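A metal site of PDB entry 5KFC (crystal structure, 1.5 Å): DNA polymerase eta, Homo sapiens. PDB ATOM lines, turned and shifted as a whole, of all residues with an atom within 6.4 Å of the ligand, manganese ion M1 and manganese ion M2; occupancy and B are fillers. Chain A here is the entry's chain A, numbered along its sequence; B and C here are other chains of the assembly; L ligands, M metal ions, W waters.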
ATOM      1  N   ASP A  16      -2.893 -28.789  18.128  1.00  0.00           N
ATOM      2  CA  ASP A  16      -3.698 -28.738  19.335  1.00  0.00           C
ATOM      3  C   ASP A  16      -3.047 -29.540  20.445  1.00  0.00           C
ATOM      4  O   ASP A  16      -2.734 -30.714  20.267  1.00  0.00           O
ATOM      5  CB  ASP A  16      -5.111 -29.258  19.084  1.00  0.00           C
ATOM      6  CG  ASP A  16      -5.942 -29.274  20.332  1.00  0.00           C
ATOM      7  OD1 ASP A  16      -5.873 -30.270  21.068  1.00  0.00           O
ATOM      8  OD2 ASP A  16      -6.661 -28.281  20.583  1.00  0.00           O
ATOM      9  N   MET A  17      -2.845 -28.914  21.596  1.00  0.00           N
ATOM     10  CA  MET A  17      -2.133 -29.580  22.679  1.00  0.00           C
ATOM     11  C   MET A  17      -2.930 -30.752  23.262  1.00  0.00           C
ATOM     12  O   MET A  17      -4.133 -30.674  23.380  1.00  0.00           O
ATOM     13  CB  MET A  17      -1.793 -28.579  23.790  1.00  0.00           C
ATOM     14  CG  MET A  17      -1.052 -27.347  23.291  1.00  0.00           C
ATOM     15  SD  MET A  17       0.463 -27.685  22.370  1.00  0.00           S
ATOM     16  CE  MET A  17       1.466 -28.392  23.620  1.00  0.00           C
ATOM     17  N   ASP A  18      -2.241 -31.839  23.616  1.00  0.00           N
ATOM     18  CA  ASP A  18      -2.937 -32.964  24.254  1.00  0.00           C
ATOM     19  C   ASP A  18      -3.239 -32.668  25.720  1.00  0.00           C
ATOM     20  O   ASP A  18      -2.334 -32.233  26.470  1.00  0.00           O
ATOM     21  CB  ASP A  18      -2.082 -34.228  24.223  1.00  0.00           C
ATOM     22  CG  ASP A  18      -1.755 -34.685  22.812  1.00  0.00           C
ATOM     23  OD1 ASP A  18      -2.514 -34.408  21.876  1.00  0.00           O
ATOM     24  OD2 ASP A  18      -0.707 -35.330  22.671  1.00  0.00           O
ATOM     25  N   CYS A  19      -4.498 -32.885  26.100  1.00  0.00           N
ATOM     26  CA  CYS A  19      -5.008 -32.686  27.474  1.00  0.00           C
ATOM     27  C   CYS A  19      -4.243 -31.544  28.154  1.00  0.00           C
ATOM     28  O   CYS A  19      -3.566 -31.742  29.155  1.00  0.00           O
ATOM     29  CB  CYS A  19      -4.958 -33.981  28.316  1.00  0.00           C
ATOM     30  SG  CYS A  19      -3.419 -34.922  28.402  1.00  0.00           S
ATOM     31  N   PHE A  20      -4.372 -30.348  27.590  1.00  0.00           N
ATOM     32  CA  PHE A  20      -3.395 -29.295  27.831  1.00  0.00           C
ATOM     33  C   PHE A  20      -3.194 -28.926  29.303  1.00  0.00           C
ATOM     34  O   PHE A  20      -2.061 -28.965  29.769  1.00  0.00           O
ATOM     35  CB  PHE A  20      -3.772 -28.020  27.036  1.00  0.00           C
ATOM     36  CG  PHE A  20      -2.760 -26.902  27.147  1.00  0.00           C
ATOM     37  CD1 PHE A  20      -1.395 -27.156  26.982  1.00  0.00           C
ATOM     38  CD2 PHE A  20      -3.162 -25.602  27.408  1.00  0.00           C
ATOM     39  CE1 PHE A  20      -0.462 -26.113  27.060  1.00  0.00           C
ATOM     40  CE2 PHE A  20      -2.221 -24.572  27.493  1.00  0.00           C
ATOM     41  CZ  PHE A  20      -0.877 -24.843  27.317  1.00  0.00           C
ATOM     42  N   PHE A  21      -4.253 -28.593  30.034  1.00  0.00           N
ATOM     43  CA  PHE A  21      -4.030 -28.151  31.409  1.00  0.00           C
ATOM     44  C   PHE A  21      -3.410 -29.280  32.250  1.00  0.00           C
ATOM     45  O   PHE A  21      -2.654 -29.023  33.179  1.00  0.00           O
ATOM     46  CB  PHE A  21      -5.312 -27.664  32.095  1.00  0.00           C
ATOM     47  CG  PHE A  21      -5.870 -26.369  31.586  1.00  0.00           C
ATOM     48  CD1 PHE A  21      -5.405 -25.774  30.402  1.00  0.00           C
ATOM     49  CD2 PHE A  21      -6.885 -25.736  32.290  1.00  0.00           C
ATOM     50  CE1 PHE A  21      -5.950 -24.572  29.955  1.00  0.00           C
ATOM     51  CE2 PHE A  21      -7.425 -24.534  31.852  1.00  0.00           C
ATOM     52  CZ  PHE A  21      -6.968 -23.956  30.673  1.00  0.00           C
ATOM     53  N   VAL A  22      -3.752 -30.530  31.926  1.00  0.00           N
ATOM     54  CA  VAL A  22      -3.149 -31.660  32.634  1.00  0.00           C
ATOM     55  C   VAL A  22      -1.650 -31.712  32.371  1.00  0.00           C
ATOM     56  O   VAL A  22      -0.849 -31.859  33.304  1.00  0.00           O
ATOM     57  CB  VAL A  22      -3.824 -32.994  32.229  1.00  0.00           C
ATOM     58  CG1 VAL A  22      -2.961 -34.189  32.648  1.00  0.00           C
ATOM     59  CG2 VAL A  22      -5.215 -33.090  32.851  1.00  0.00           C
ATOM     60  N   GLN A  41     -11.543 -27.250  39.064  1.00  0.00           N
ATOM     61  CA  GLN A  41     -11.623 -25.912  39.663  1.00  0.00           C
ATOM     62  C   GLN A  41     -12.690 -25.906  40.743  1.00  0.00           C
ATOM     63  O   GLN A  41     -13.791 -26.456  40.587  1.00  0.00           O
ATOM     64  CB  GLN A  41     -11.847 -24.811  38.611  1.00  0.00           C
ATOM     65  CG  GLN A  41     -13.001 -24.963  37.668  1.00  0.00           C
ATOM     66  CD  GLN A  41     -12.970 -23.922  36.533  1.00  0.00           C
ATOM     67  OE1 GLN A  41     -12.043 -23.101  36.410  1.00  0.00           O
ATOM     68  NE2 GLN A  41     -13.998 -23.959  35.711  1.00  0.00           N
ATOM     69  N   ILE A  51     -12.071 -29.861  34.347  1.00  0.00           N
ATOM     70  CA  ILE A  51     -11.973 -29.145  33.070  1.00  0.00           C
ATOM     71  C   ILE A  51     -10.920 -29.728  32.126  1.00  0.00           C
ATOM     72  O   ILE A  51     -10.856 -29.331  30.976  1.00  0.00           O
ATOM     73  CB  ILE A  51     -11.681 -27.637  33.272  1.00  0.00           C
ATOM     74  CG1 ILE A  51     -10.368 -27.398  34.029  1.00  0.00           C
ATOM     75  CG2 ILE A  51     -12.872 -26.961  33.961  1.00  0.00           C
ATOM     76  CD1 ILE A  51      -9.945 -25.925  34.062  1.00  0.00           C
ATOM     77  N   ALA A  52     -10.132 -30.701  32.583  1.00  0.00           N
ATOM     78  CA  ALA A  52      -9.172 -31.380  31.700  1.00  0.00           C
ATOM     79  C   ALA A  52      -8.854 -32.760  32.270  1.00  0.00           C
ATOM     80  O   ALA A  52      -8.810 -32.916  33.495  1.00  0.00           O
ATOM     81  CB  ALA A  52      -7.872 -30.561  31.537  1.00  0.00           C
ATOM     82  N   VAL A  53      -8.605 -33.738  31.395  1.00  0.00           N
ATOM     83  CA  VAL A  53      -8.507 -35.156  31.786  1.00  0.00           C
ATOM     84  C   VAL A  53      -7.386 -35.852  31.036  1.00  0.00           C
ATOM     85  O   VAL A  53      -7.355 -35.789  29.798  1.00  0.00           O
ATOM     86  CB  VAL A  53      -9.830 -35.917  31.498  1.00  0.00           C
ATOM     87  CG1 VAL A  53      -9.775 -37.336  32.061  1.00  0.00           C
ATOM     88  CG2 VAL A  53     -11.019 -35.193  32.090  1.00  0.00           C
ATOM     89  N   TYR A  55      -5.262 -38.955  29.361  1.00  0.00           N
ATOM     90  CA  TYR A  55      -5.775 -40.062  28.565  1.00  0.00           C
ATOM     91  C   TYR A  55      -5.893 -41.327  29.398  1.00  0.00           C
ATOM     92  O   TYR A  55      -6.815 -42.127  29.182  1.00  0.00           O
ATOM     93  CB  TYR A  55      -4.904 -40.248  27.313  1.00  0.00           C
ATOM     94  CG  TYR A  55      -5.285 -39.225  26.268  1.00  0.00           C
ATOM     95  CD1 TYR A  55      -4.793 -37.924  26.326  1.00  0.00           C
ATOM     96  CD2 TYR A  55      -6.192 -39.536  25.258  1.00  0.00           C
ATOM     97  CE1 TYR A  55      -5.175 -36.959  25.389  1.00  0.00           C
ATOM     98  CE2 TYR A  55      -6.563 -38.603  24.312  1.00  0.00           C
ATOM     99  CZ  TYR A  55      -6.070 -37.311  24.382  1.00  0.00           C
ATOM    100  OH  TYR A  55      -6.449 -36.367  23.454  1.00  0.00           O
ATOM    101  N   ARG A  58      -9.209 -40.969  31.006  1.00  0.00           N
ATOM    102  CA  ARG A  58     -10.305 -41.118  30.061  1.00  0.00           C
ATOM    103  C   ARG A  58     -10.673 -42.591  29.873  1.00  0.00           C
ATOM    104  O   ARG A  58     -11.835 -42.893  29.615  1.00  0.00           O
ATOM    105  CB  ARG A  58      -9.968 -40.502  28.699  1.00  0.00           C
ATOM    106  CG  ARG A  58      -9.720 -39.014  28.775  1.00  0.00           C
ATOM    107  CD  ARG A  58      -9.435 -38.407  27.410  1.00  0.00           C
ATOM    108  NE  ARG A  58      -8.874 -37.066  27.591  1.00  0.00           N
ATOM    109  CZ  ARG A  58      -8.703 -36.173  26.626  1.00  0.00           C
ATOM    110  NH1 ARG A  58      -9.051 -36.466  25.382  1.00  0.00           N
ATOM    111  NH2 ARG A  58      -8.176 -34.975  26.923  1.00  0.00           N
ATOM    112  N   ARG A  64     -14.479 -34.172  30.967  1.00  0.00           N
ATOM    113  CA  ARG A  64     -14.730 -32.780  31.285  1.00  0.00           C
ATOM    114  C   ARG A  64     -16.187 -32.577  31.737  1.00  0.00           C
ATOM    115  O   ARG A  64     -17.074 -33.320  31.331  1.00  0.00           O
ATOM    116  CB  ARG A  64     -14.413 -31.917  30.056  1.00  0.00           C
ATOM    117  CG  ARG A  64     -14.804 -30.462  30.132  1.00  0.00           C
ATOM    118  CD  ARG A  64     -14.266 -29.727  28.913  1.00  0.00           C
ATOM    119  NE  ARG A  64     -12.811 -29.780  28.953  1.00  0.00           N
ATOM    120  CZ  ARG A  64     -12.025 -30.081  27.923  1.00  0.00           C
ATOM    121  NH1 ARG A  64     -12.527 -30.339  26.708  1.00  0.00           N
ATOM    122  NH2 ARG A  64     -10.715 -30.112  28.106  1.00  0.00           N
ATOM    123  N   LEU A  92      -6.541 -18.351  35.717  1.00  0.00           N
ATOM    124  CA  LEU A  92      -6.000 -19.252  34.699  1.00  0.00           C
ATOM    125  C   LEU A  92      -4.630 -18.808  34.153  1.00  0.00           C
ATOM    126  O   LEU A  92      -4.215 -19.264  33.090  1.00  0.00           O
ATOM    127  CB  LEU A  92      -6.983 -19.384  33.537  1.00  0.00           C
ATOM    128  CG  LEU A  92      -8.402 -19.801  33.912  1.00  0.00           C
ATOM    129  CD1 LEU A  92      -9.299 -19.729  32.683  1.00  0.00           C
ATOM    130  CD2 LEU A  92      -8.392 -21.228  34.480  1.00  0.00           C
ATOM    131  N   SER A 116      -7.528 -20.946  20.201  1.00  0.00           N
ATOM    132  CA  SER A 116      -7.909 -21.196  21.583  1.00  0.00           C
ATOM    133  C   SER A 116      -6.683 -21.104  22.467  1.00  0.00           C
ATOM    134  O   SER A 116      -5.577 -20.887  21.985  1.00  0.00           O
ATOM    135  CB  SER A 116      -8.556 -22.582  21.757  1.00  0.00           C
ATOM    136  OG  SER A 116      -7.585 -23.602  21.855  1.00  0.00           O
ATOM    137  N   ILE A 117      -6.865 -21.329  23.755  1.00  0.00           N
ATOM    138  CA  ILE A 117      -5.730 -21.326  24.650  1.00  0.00           C
ATOM    139  C   ILE A 117      -4.729 -22.429  24.286  1.00  0.00           C
ATOM    140  O   ILE A 117      -3.559 -22.339  24.633  1.00  0.00           O
ATOM    141  CB  ILE A 117      -6.186 -21.478  26.130  1.00  0.00           C
ATOM    142  CG1 ILE A 117      -5.079 -21.010  27.083  1.00  0.00           C
ATOM    143  CG2 ILE A 117      -6.638 -22.911  26.438  1.00  0.00           C
ATOM    144  CD1 ILE A 117      -5.586 -20.809  28.503  1.00  0.00           C
ATOM    145  N   ASP A 118      -5.150 -23.481  23.586  1.00  0.00           N
ATOM    146  CA  ASP A 118      -4.206 -24.561  23.367  1.00  0.00           C
ATOM    147  C   ASP A 118      -4.105 -24.986  21.899  1.00  0.00           C
ATOM    148  O   ASP A 118      -3.604 -26.091  21.600  1.00  0.00           O
ATOM    149  CB  ASP A 118      -4.563 -25.778  24.236  1.00  0.00           C
ATOM    150  CG  ASP A 118      -5.571 -26.707  23.586  1.00  0.00           C
ATOM    151  OD1 ASP A 118      -6.506 -26.250  22.886  1.00  0.00           O
ATOM    152  OD2 ASP A 118      -5.348 -27.946  23.694  1.00  0.00           O
ATOM    153  N   GLU A 119      -4.534 -24.132  20.980  1.00  0.00           N
ATOM    154  CA  GLU A 119      -4.380 -24.504  19.574  1.00  0.00           C
ATOM    155  C   GLU A 119      -4.260 -23.322  18.644  1.00  0.00           C
ATOM    156  O   GLU A 119      -4.742 -22.219  18.932  1.00  0.00           O
ATOM    157  CB  GLU A 119      -5.536 -25.376  19.128  1.00  0.00           C
ATOM    158  CG  GLU A 119      -6.797 -24.638  18.859  1.00  0.00           C
ATOM    159  CD  GLU A 119      -7.999 -25.523  19.053  1.00  0.00           C
ATOM    160  OE1 GLU A 119      -8.563 -25.992  18.056  1.00  0.00           O
ATOM    161  OE2 GLU A 119      -8.367 -25.760  20.223  1.00  0.00           O
ATOM    162  N   SER A 216      -1.115 -32.899  19.169  1.00  0.00           N
ATOM    163  CA  SER A 216      -1.516 -33.542  17.932  1.00  0.00           C
ATOM    164  C   SER A 216      -1.649 -32.486  16.856  1.00  0.00           C
ATOM    165  O   SER A 216      -1.631 -31.289  17.140  1.00  0.00           O
ATOM    166  CB  SER A 216      -2.816 -34.300  18.131  1.00  0.00           C
ATOM    167  OG  SER A 216      -2.652 -35.304  19.128  1.00  0.00           O
ATOM    168  N   LYS A 227      -8.606 -29.097  11.322  1.00  0.00           N
ATOM    169  CA  LYS A 227      -9.159 -29.320  12.650  1.00  0.00           C
ATOM    170  C   LYS A 227      -9.723 -30.737  12.793  1.00  0.00           C
ATOM    171  O   LYS A 227      -9.478 -31.430  13.786  1.00  0.00           O
ATOM    172  CB  LYS A 227     -10.258 -28.283  12.946  1.00  0.00           C
ATOM    173  CG  LYS A 227     -10.926 -28.465  14.313  1.00  0.00           C
ATOM    174  CD  LYS A 227      -9.914 -28.464  15.456  1.00  0.00           C
ATOM    175  CE  LYS A 227     -10.610 -28.541  16.807  1.00  0.00           C
ATOM    176  NZ  LYS A 227      -9.687 -28.471  17.972  1.00  0.00           N
ATOM    177  N   LYS A 234      -5.449 -38.510  17.862  1.00  0.00           N
ATOM    178  CA  LYS A 234      -4.911 -38.078  19.186  1.00  0.00           C
ATOM    179  C   LYS A 234      -4.729 -39.257  20.157  1.00  0.00           C
ATOM    180  O   LYS A 234      -5.547 -40.125  20.112  1.00  0.00           O
ATOM    181  CB  LYS A 234      -5.902 -37.114  19.817  1.00  0.00           C
ATOM    182  CG  LYS A 234      -5.676 -35.688  19.477  1.00  0.00           C
ATOM    183  CD  LYS A 234      -6.377 -34.639  20.361  1.00  0.00           C
ATOM    184  CE  LYS A 234      -5.866 -33.192  20.015  1.00  0.00           C
ATOM    185  NZ  LYS A 234      -4.994 -32.817  21.156  1.00  0.00           N
ATOM    186  N   PRO A 235      -3.868 -39.194  21.172  1.00  0.00           N
ATOM    187  CA  PRO A 235      -2.908 -38.106  21.281  1.00  0.00           C
ATOM    188  C   PRO A 235      -1.531 -38.338  20.654  1.00  0.00           C
ATOM    189  O   PRO A 235      -1.248 -39.382  20.258  1.00  0.00           O
ATOM    190  CB  PRO A 235      -2.723 -37.999  22.798  1.00  0.00           C
ATOM    191  CG  PRO A 235      -2.723 -39.380  23.278  1.00  0.00           C
ATOM    192  CD  PRO A 235      -3.622 -40.125  22.402  1.00  0.00           C
ATOM    193  P    DT B   8     -13.509 -25.948  18.709  1.00  0.00           P
ATOM    194  OP1  DT B   8     -13.244 -24.681  18.008  1.00  0.00           O
ATOM    195  OP2  DT B   8     -13.155 -27.233  18.074  1.00  0.00           O
ATOM    196  O5'  DT B   8     -12.805 -25.933  20.125  1.00  0.00           O
ATOM    197  C5'  DT B   8     -11.826 -25.029  20.352  1.00  0.00           C
ATOM    198  C4'  DT B   8     -11.486 -24.926  21.827  1.00  0.00           C
ATOM    199  O4'  DT B   8     -12.517 -24.291  22.613  1.00  0.00           O
ATOM    200  C3'  DT B   8     -11.070 -26.183  22.597  1.00  0.00           C
ATOM    201  O3'  DT B   8      -9.700 -26.103  22.956  1.00  0.00           O
ATOM    202  C2'  DT B   8     -12.010 -26.208  23.820  1.00  0.00           C
ATOM    203  C1'  DT B   8     -12.437 -24.756  23.931  1.00  0.00           C
ATOM    204  N1   DT B   8     -13.759 -24.577  24.594  1.00  0.00           N
ATOM    205  C2   DT B   8     -13.848 -23.782  25.709  1.00  0.00           C
ATOM    206  O2   DT B   8     -12.898 -23.226  26.192  1.00  0.00           O
ATOM    207  N3   DT B   8     -15.115 -23.687  26.252  1.00  0.00           N
ATOM    208  C4   DT B   8     -16.270 -24.280  25.784  1.00  0.00           C
ATOM    209  O4   DT B   8     -17.352 -24.140  26.337  1.00  0.00           O
ATOM    210  C5   DT B   8     -16.098 -25.097  24.602  1.00  0.00           C
ATOM    211  C7   DT B   8     -17.282 -25.794  23.997  1.00  0.00           C
ATOM    212  C6   DT B   8     -14.871 -25.200  24.074  1.00  0.00           C
ATOM    213  P    DT C   3     -25.043 -28.339  37.021  1.00  0.00           P
ATOM    214  OP1  DT C   3     -26.231 -27.642  36.477  1.00  0.00           O
ATOM    215  OP2  DT C   3     -25.113 -29.765  37.402  1.00  0.00           O
ATOM    216  O5'  DT C   3     -23.843 -28.140  35.987  1.00  0.00           O
ATOM    217  C5'  DT C   3     -22.519 -28.454  36.373  1.00  0.00           C
ATOM    218  C4'  DT C   3     -21.517 -27.803  35.437  1.00  0.00           C
ATOM    219  O4'  DT C   3     -21.363 -28.622  34.254  1.00  0.00           O
ATOM    220  C3'  DT C   3     -21.941 -26.407  34.948  1.00  0.00           C
ATOM    221  O3'  DT C   3     -20.947 -25.450  35.285  1.00  0.00           O
ATOM    222  C2'  DT C   3     -22.122 -26.573  33.440  1.00  0.00           C
ATOM    223  C1'  DT C   3     -21.267 -27.794  33.123  1.00  0.00           C
ATOM    224  N1   DT C   3     -21.754 -28.569  31.954  1.00  0.00           N
ATOM    225  C2   DT C   3     -20.905 -28.782  30.895  1.00  0.00           C
ATOM    226  O2   DT C   3     -19.766 -28.368  30.858  1.00  0.00           O
ATOM    227  N3   DT C   3     -21.448 -29.512  29.870  1.00  0.00           N
ATOM    228  C4   DT C   3     -22.721 -30.036  29.791  1.00  0.00           C
ATOM    229  O4   DT C   3     -23.116 -30.681  28.826  1.00  0.00           O
ATOM    230  C5   DT C   3     -23.559 -29.773  30.938  1.00  0.00           C
ATOM    231  C7   DT C   3     -24.975 -30.286  30.976  1.00  0.00           C
ATOM    232  C6   DT C   3     -23.049 -29.055  31.948  1.00  0.00           C
ATOM    233  P    DT C   4     -21.345 -24.194  36.211  1.00  0.00           P
ATOM    234  OP1  DT C   4     -21.820 -24.732  37.510  1.00  0.00           O
ATOM    235  OP2  DT C   4     -22.239 -23.353  35.380  1.00  0.00           O
ATOM    236  O5'  DT C   4     -19.981 -23.371  36.401  1.00  0.00           O
ATOM    237  C5'  DT C   4     -19.046 -23.682  37.448  1.00  0.00           C
ATOM    238  C4'  DT C   4     -17.707 -23.028  37.151  1.00  0.00           C
ATOM    239  O4'  DT C   4     -17.182 -23.605  35.943  1.00  0.00           O
ATOM    240  C3'  DT C   4     -17.756 -21.524  36.908  1.00  0.00           C
ATOM    241  O3'  DT C   4     -16.545 -20.950  37.375  1.00  0.00           O
ATOM    242  C2'  DT C   4     -17.880 -21.431  35.377  1.00  0.00           C
ATOM    243  C1'  DT C   4     -16.984 -22.590  34.961  1.00  0.00           C
ATOM    244  N1   DT C   4     -17.268 -23.211  33.661  1.00  0.00           N
ATOM    245  C2   DT C   4     -16.198 -23.644  32.934  1.00  0.00           C
ATOM    246  O2   DT C   4     -15.046 -23.457  33.293  1.00  0.00           O
ATOM    247  N3   DT C   4     -16.507 -24.256  31.758  1.00  0.00           N
ATOM    248  C4   DT C   4     -17.757 -24.522  31.259  1.00  0.00           C
ATOM    249  O4   DT C   4     -17.920 -25.093  30.190  1.00  0.00           O
ATOM    250  C5   DT C   4     -18.854 -24.064  32.087  1.00  0.00           C
ATOM    251  C7   DT C   4     -20.278 -24.288  31.642  1.00  0.00           C
ATOM    252  C6   DT C   4     -18.560 -23.460  33.249  1.00  0.00           C
ATOM    253  P    DA C   5     -16.286 -19.374  37.277  1.00  0.00           P
ATOM    254  OP1  DA C   5     -15.550 -19.012  38.507  1.00  0.00           O
ATOM    255  OP2  DA C   5     -17.532 -18.693  36.902  1.00  0.00           O
ATOM    256  O5'  DA C   5     -15.282 -19.243  36.048  1.00  0.00           O
ATOM    257  C5'  DA C   5     -13.975 -19.784  36.133  1.00  0.00           C
ATOM    258  C4'  DA C   5     -13.180 -19.449  34.888  1.00  0.00           C
ATOM    259  O4'  DA C   5     -13.667 -20.235  33.754  1.00  0.00           O
ATOM    260  C3'  DA C   5     -13.285 -17.983  34.453  1.00  0.00           C
ATOM    261  O3'  DA C   5     -12.034 -17.579  33.949  1.00  0.00           O
ATOM    262  C2'  DA C   5     -14.342 -18.041  33.352  1.00  0.00           C
ATOM    263  C1'  DA C   5     -13.993 -19.359  32.684  1.00  0.00           C
ATOM    264  N9   DA C   5     -15.072 -19.940  31.927  1.00  0.00           N
ATOM    265  C8   DA C   5     -16.408 -19.884  32.216  1.00  0.00           C
ATOM    266  N7   DA C   5     -17.159 -20.539  31.351  1.00  0.00           N
ATOM    267  C5   DA C   5     -16.247 -21.065  30.453  1.00  0.00           C
ATOM    268  C6   DA C   5     -16.404 -21.856  29.307  1.00  0.00           C
ATOM    269  N6   DA C   5     -17.590 -22.270  28.861  1.00  0.00           N
ATOM    270  N1   DA C   5     -15.290 -22.214  28.624  1.00  0.00           N
ATOM    271  C2   DA C   5     -14.098 -21.800  29.078  1.00  0.00           C
ATOM    272  N3   DA C   5     -13.825 -21.051  30.148  1.00  0.00           N
ATOM    273  C4   DA C   5     -14.962 -20.715  30.798  1.00  0.00           C
HETATM  274  P1  LIG L   1      -7.464 -33.028  24.023  1.00  0.00           P
HETATM  275  O1  LIG L   1      -7.337 -31.851  23.089  1.00  0.00           O
HETATM  276  O2  LIG L   1      -6.220 -33.880  24.076  1.00  0.00           O
HETATM  277  O3  LIG L   1      -8.699 -33.888  23.725  1.00  0.00           O
HETATM  278  P2  LIG L   1      -7.699 -30.943  25.973  1.00  0.00           P
HETATM  279  O4  LIG L   1      -6.454 -30.256  25.451  1.00  0.00           O
HETATM  280  O5  LIG L   1      -7.780 -30.896  27.484  1.00  0.00           O
HETATM  281  O6  LIG L   1      -7.691 -32.491  25.514  1.00  0.00           O
HETATM  282  P3  LIG L   1      -9.267 -28.995  24.528  1.00  0.00           P
HETATM  283  O7  LIG L   1      -8.344 -28.822  23.364  1.00  0.00           O
HETATM  284  O8  LIG L   1     -10.738 -29.059  24.127  1.00  0.00           O
HETATM  285  O9  LIG L   1      -9.026 -30.341  25.352  1.00  0.00           O
HETATM  286  O10 LIG L   1      -9.119 -27.809  25.563  1.00  0.00           O
HETATM  287  C1  LIG L   1      -7.863 -27.290  25.905  1.00  0.00           C
HETATM  288  C2  LIG L   1      -7.872 -26.781  27.348  1.00  0.00           C
HETATM  289  O11 LIG L   1      -8.830 -25.752  27.432  1.00  0.00           O
HETATM  290  C3  LIG L   1      -8.252 -27.816  28.293  1.00  0.00           C
HETATM  291  O12 LIG L   1      -7.107 -28.573  28.734  1.00  0.00           O
HETATM  292  C4  LIG L   1      -8.898 -27.080  29.391  1.00  0.00           C
HETATM  293  C5  LIG L   1      -9.519 -25.917  28.682  1.00  0.00           C
HETATM  294  N1  LIG L   1     -10.903 -26.112  28.415  1.00  0.00           N
HETATM  295  C6  LIG L   1     -11.465 -26.755  27.367  1.00  0.00           C
HETATM  296  N2  LIG L   1     -12.791 -26.747  27.469  1.00  0.00           N
HETATM  297  C7  LIG L   1     -13.124 -26.058  28.577  1.00  0.00           C
HETATM  298  C8  LIG L   1     -14.315 -25.714  29.202  1.00  0.00           C
HETATM  299  N3  LIG L   1     -15.564 -26.102  28.630  1.00  0.00           N
HETATM  300  N4  LIG L   1     -14.277 -25.015  30.342  1.00  0.00           N
HETATM  301  C9  LIG L   1     -13.122 -24.623  30.916  1.00  0.00           C
HETATM  302  N5  LIG L   1     -11.936 -24.951  30.329  1.00  0.00           N
HETATM  303  C10 LIG L   1     -11.926 -25.655  29.182  1.00  0.00           C
HETATM  304 MN    MN M   1      -6.197 -29.930  23.206  1.00  0.00          MN
HETATM  305 MN    MN M   2      -8.098 -27.321  21.733  1.00  0.00          MN
HETATM  306  O   HOH W   1     -10.301 -22.941  31.438  1.00  0.00           O
HETATM  307  O   HOH W   2      -9.278 -24.587  24.950  1.00  0.00           O
HETATM  308  O   HOH W   3     -10.549 -22.783  27.479  1.00  0.00           O
HETATM  309  O   HOH W   4      -9.198 -31.427  21.155  1.00  0.00           O
HETATM  310  O   HOH W   5      -9.625 -28.645  20.845  1.00  0.00           O
HETATM  311  O   HOH W   6     -15.053 -27.927  26.251  1.00  0.00           O
HETATM  312  O   HOH W   7      -9.064 -32.943  28.726  1.00  0.00           O
HETATM  313  O   HOH W   8     -11.147 -33.539  24.754  1.00  0.00           O
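O3' of DT 8 of chain B lies close to OG of Ser 116, 3.5 Å away. OP2 of DT 8 of chain B is in salt-bridge range of NZ of Lys 227 (3.7 Å). N of Asp 118 lies within hydrogen-bond range of OG of Ser 116, at 3.0 Å. O of Met 17 lies close to NZ of Lys 234 (3.2 Å). The backbone carbonyl oxygen (O) of Asp 16 lies within hydrogen-bond range of the side-chain amino group (NZ) of Lys 234, at 3.2 Å. O2 of DT 4 of chain C is in hydrogen-bond range of the side-chain amide nitrogen (NE2) of Gln 41. NZ of Lys 234 lies within salt-bridge range of OD1 of Asp 18, at 3.0 Å. The side-chain hydroxyl of Ser 216 is in hydrogen-bond range of the side-chain carboxylate of Asp 18, at 2.9 Å.
N1 of DA 5 of chain C sits close to N4 of the ligand, 3.4 Å away. Asp 18 touches the ligand. O of Ile 51 touches C4 of the ligand, 3.4 Å away. CB of Ala 52 touches O12 of the ligand, at 3.5 Å. Ile 117 touches the ligand (CG2 to O11, 3.7 Å). Of the 27 residues printed, 17 come within 4 Å of the ligand.
OG of Ser 116 touches manganese ion M2, at 3.8 Å. Of the 27 residues printed, 5 come within 4 Å of manganese ion M2. The nearest printed residue that does not touch manganese ion M2 is Lys 227 (4.2 Å).
Manganese ion M2 is bound by OD2 of Asp 16 (2.1 Å), OE2 of Glu 119 (2.2 Å), water W5 (2.2 Å), O7 of the ligand (2.2 Å), OD1 of Asp 118 (2.2 Å) and O3' of DT 8 of chain B (2.4 Å).
Lys 234 touches manganese ion M1. Four residues have an atom within 4 Å of manganese ion M1: Asp 16, Met 17, Asp 118 and Lys 234. Along chain A the residues within 4 Å of manganese ion M1 span positions 16 to 234. The nearest printed residue that does not touch manganese ion M1 is Asp 18 (4.4 Å).
The side-chain hydroxyl of Tyr 55 is in hydrogen-bond range of an oxygen (O2) of the ligand (2.6 Å). O2 of the ligand is in hydrogen-bond range of N of Cys 19 (2.8 Å). N3 of the ligand sits at hydrogen-bond distance from N3 of DT 8 of chain B (3.4 Å). N of Phe 21 lies within hydrogen-bond range of O12 of the ligand (3.1 Å). An oxygen (O5) of the ligand lies within salt-bridge range of the guanidinium group of Arg 64 (3.1 Å). O3 of the ligand lies within salt-bridge range of NH1 of Arg 58, 3.1 Å away. An oxygen (O5) of the ligand is in hydrogen-bond range of the backbone NH of Phe 20 (3.5 Å). NZ of Lys 234 is in salt-bridge range of O2 of the ligand, 3.3 Å away. O4 of DT 4 of chain C sits at hydrogen-bond distance from a nitrogen (N3) of the ligand, 3.0 Å away.
Water W5 lies within hydrogen-bond range of the side-chain amino group (NZ) of Lys 227 (2.9 Å) and an oxygen (O8) of the ligand (3.5 Å). Water W3 lies within hydrogen-bond range of O2 of DT 8 of chain B (2.7 Å) and an oxygen (O11) of the ligand (3.4 Å).
Manganese ion M1 is bound by OD1 of Asp 16 (2.2 Å), O of Met 17 (2.2 Å), OD2 of Asp 118 (2.2 Å), O1 of the ligand (2.2 Å), O4 of the ligand (2.3 Å) and O7 of the ligand (2.4 Å). Manganese ion M1 has six donor atoms within binding distance.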
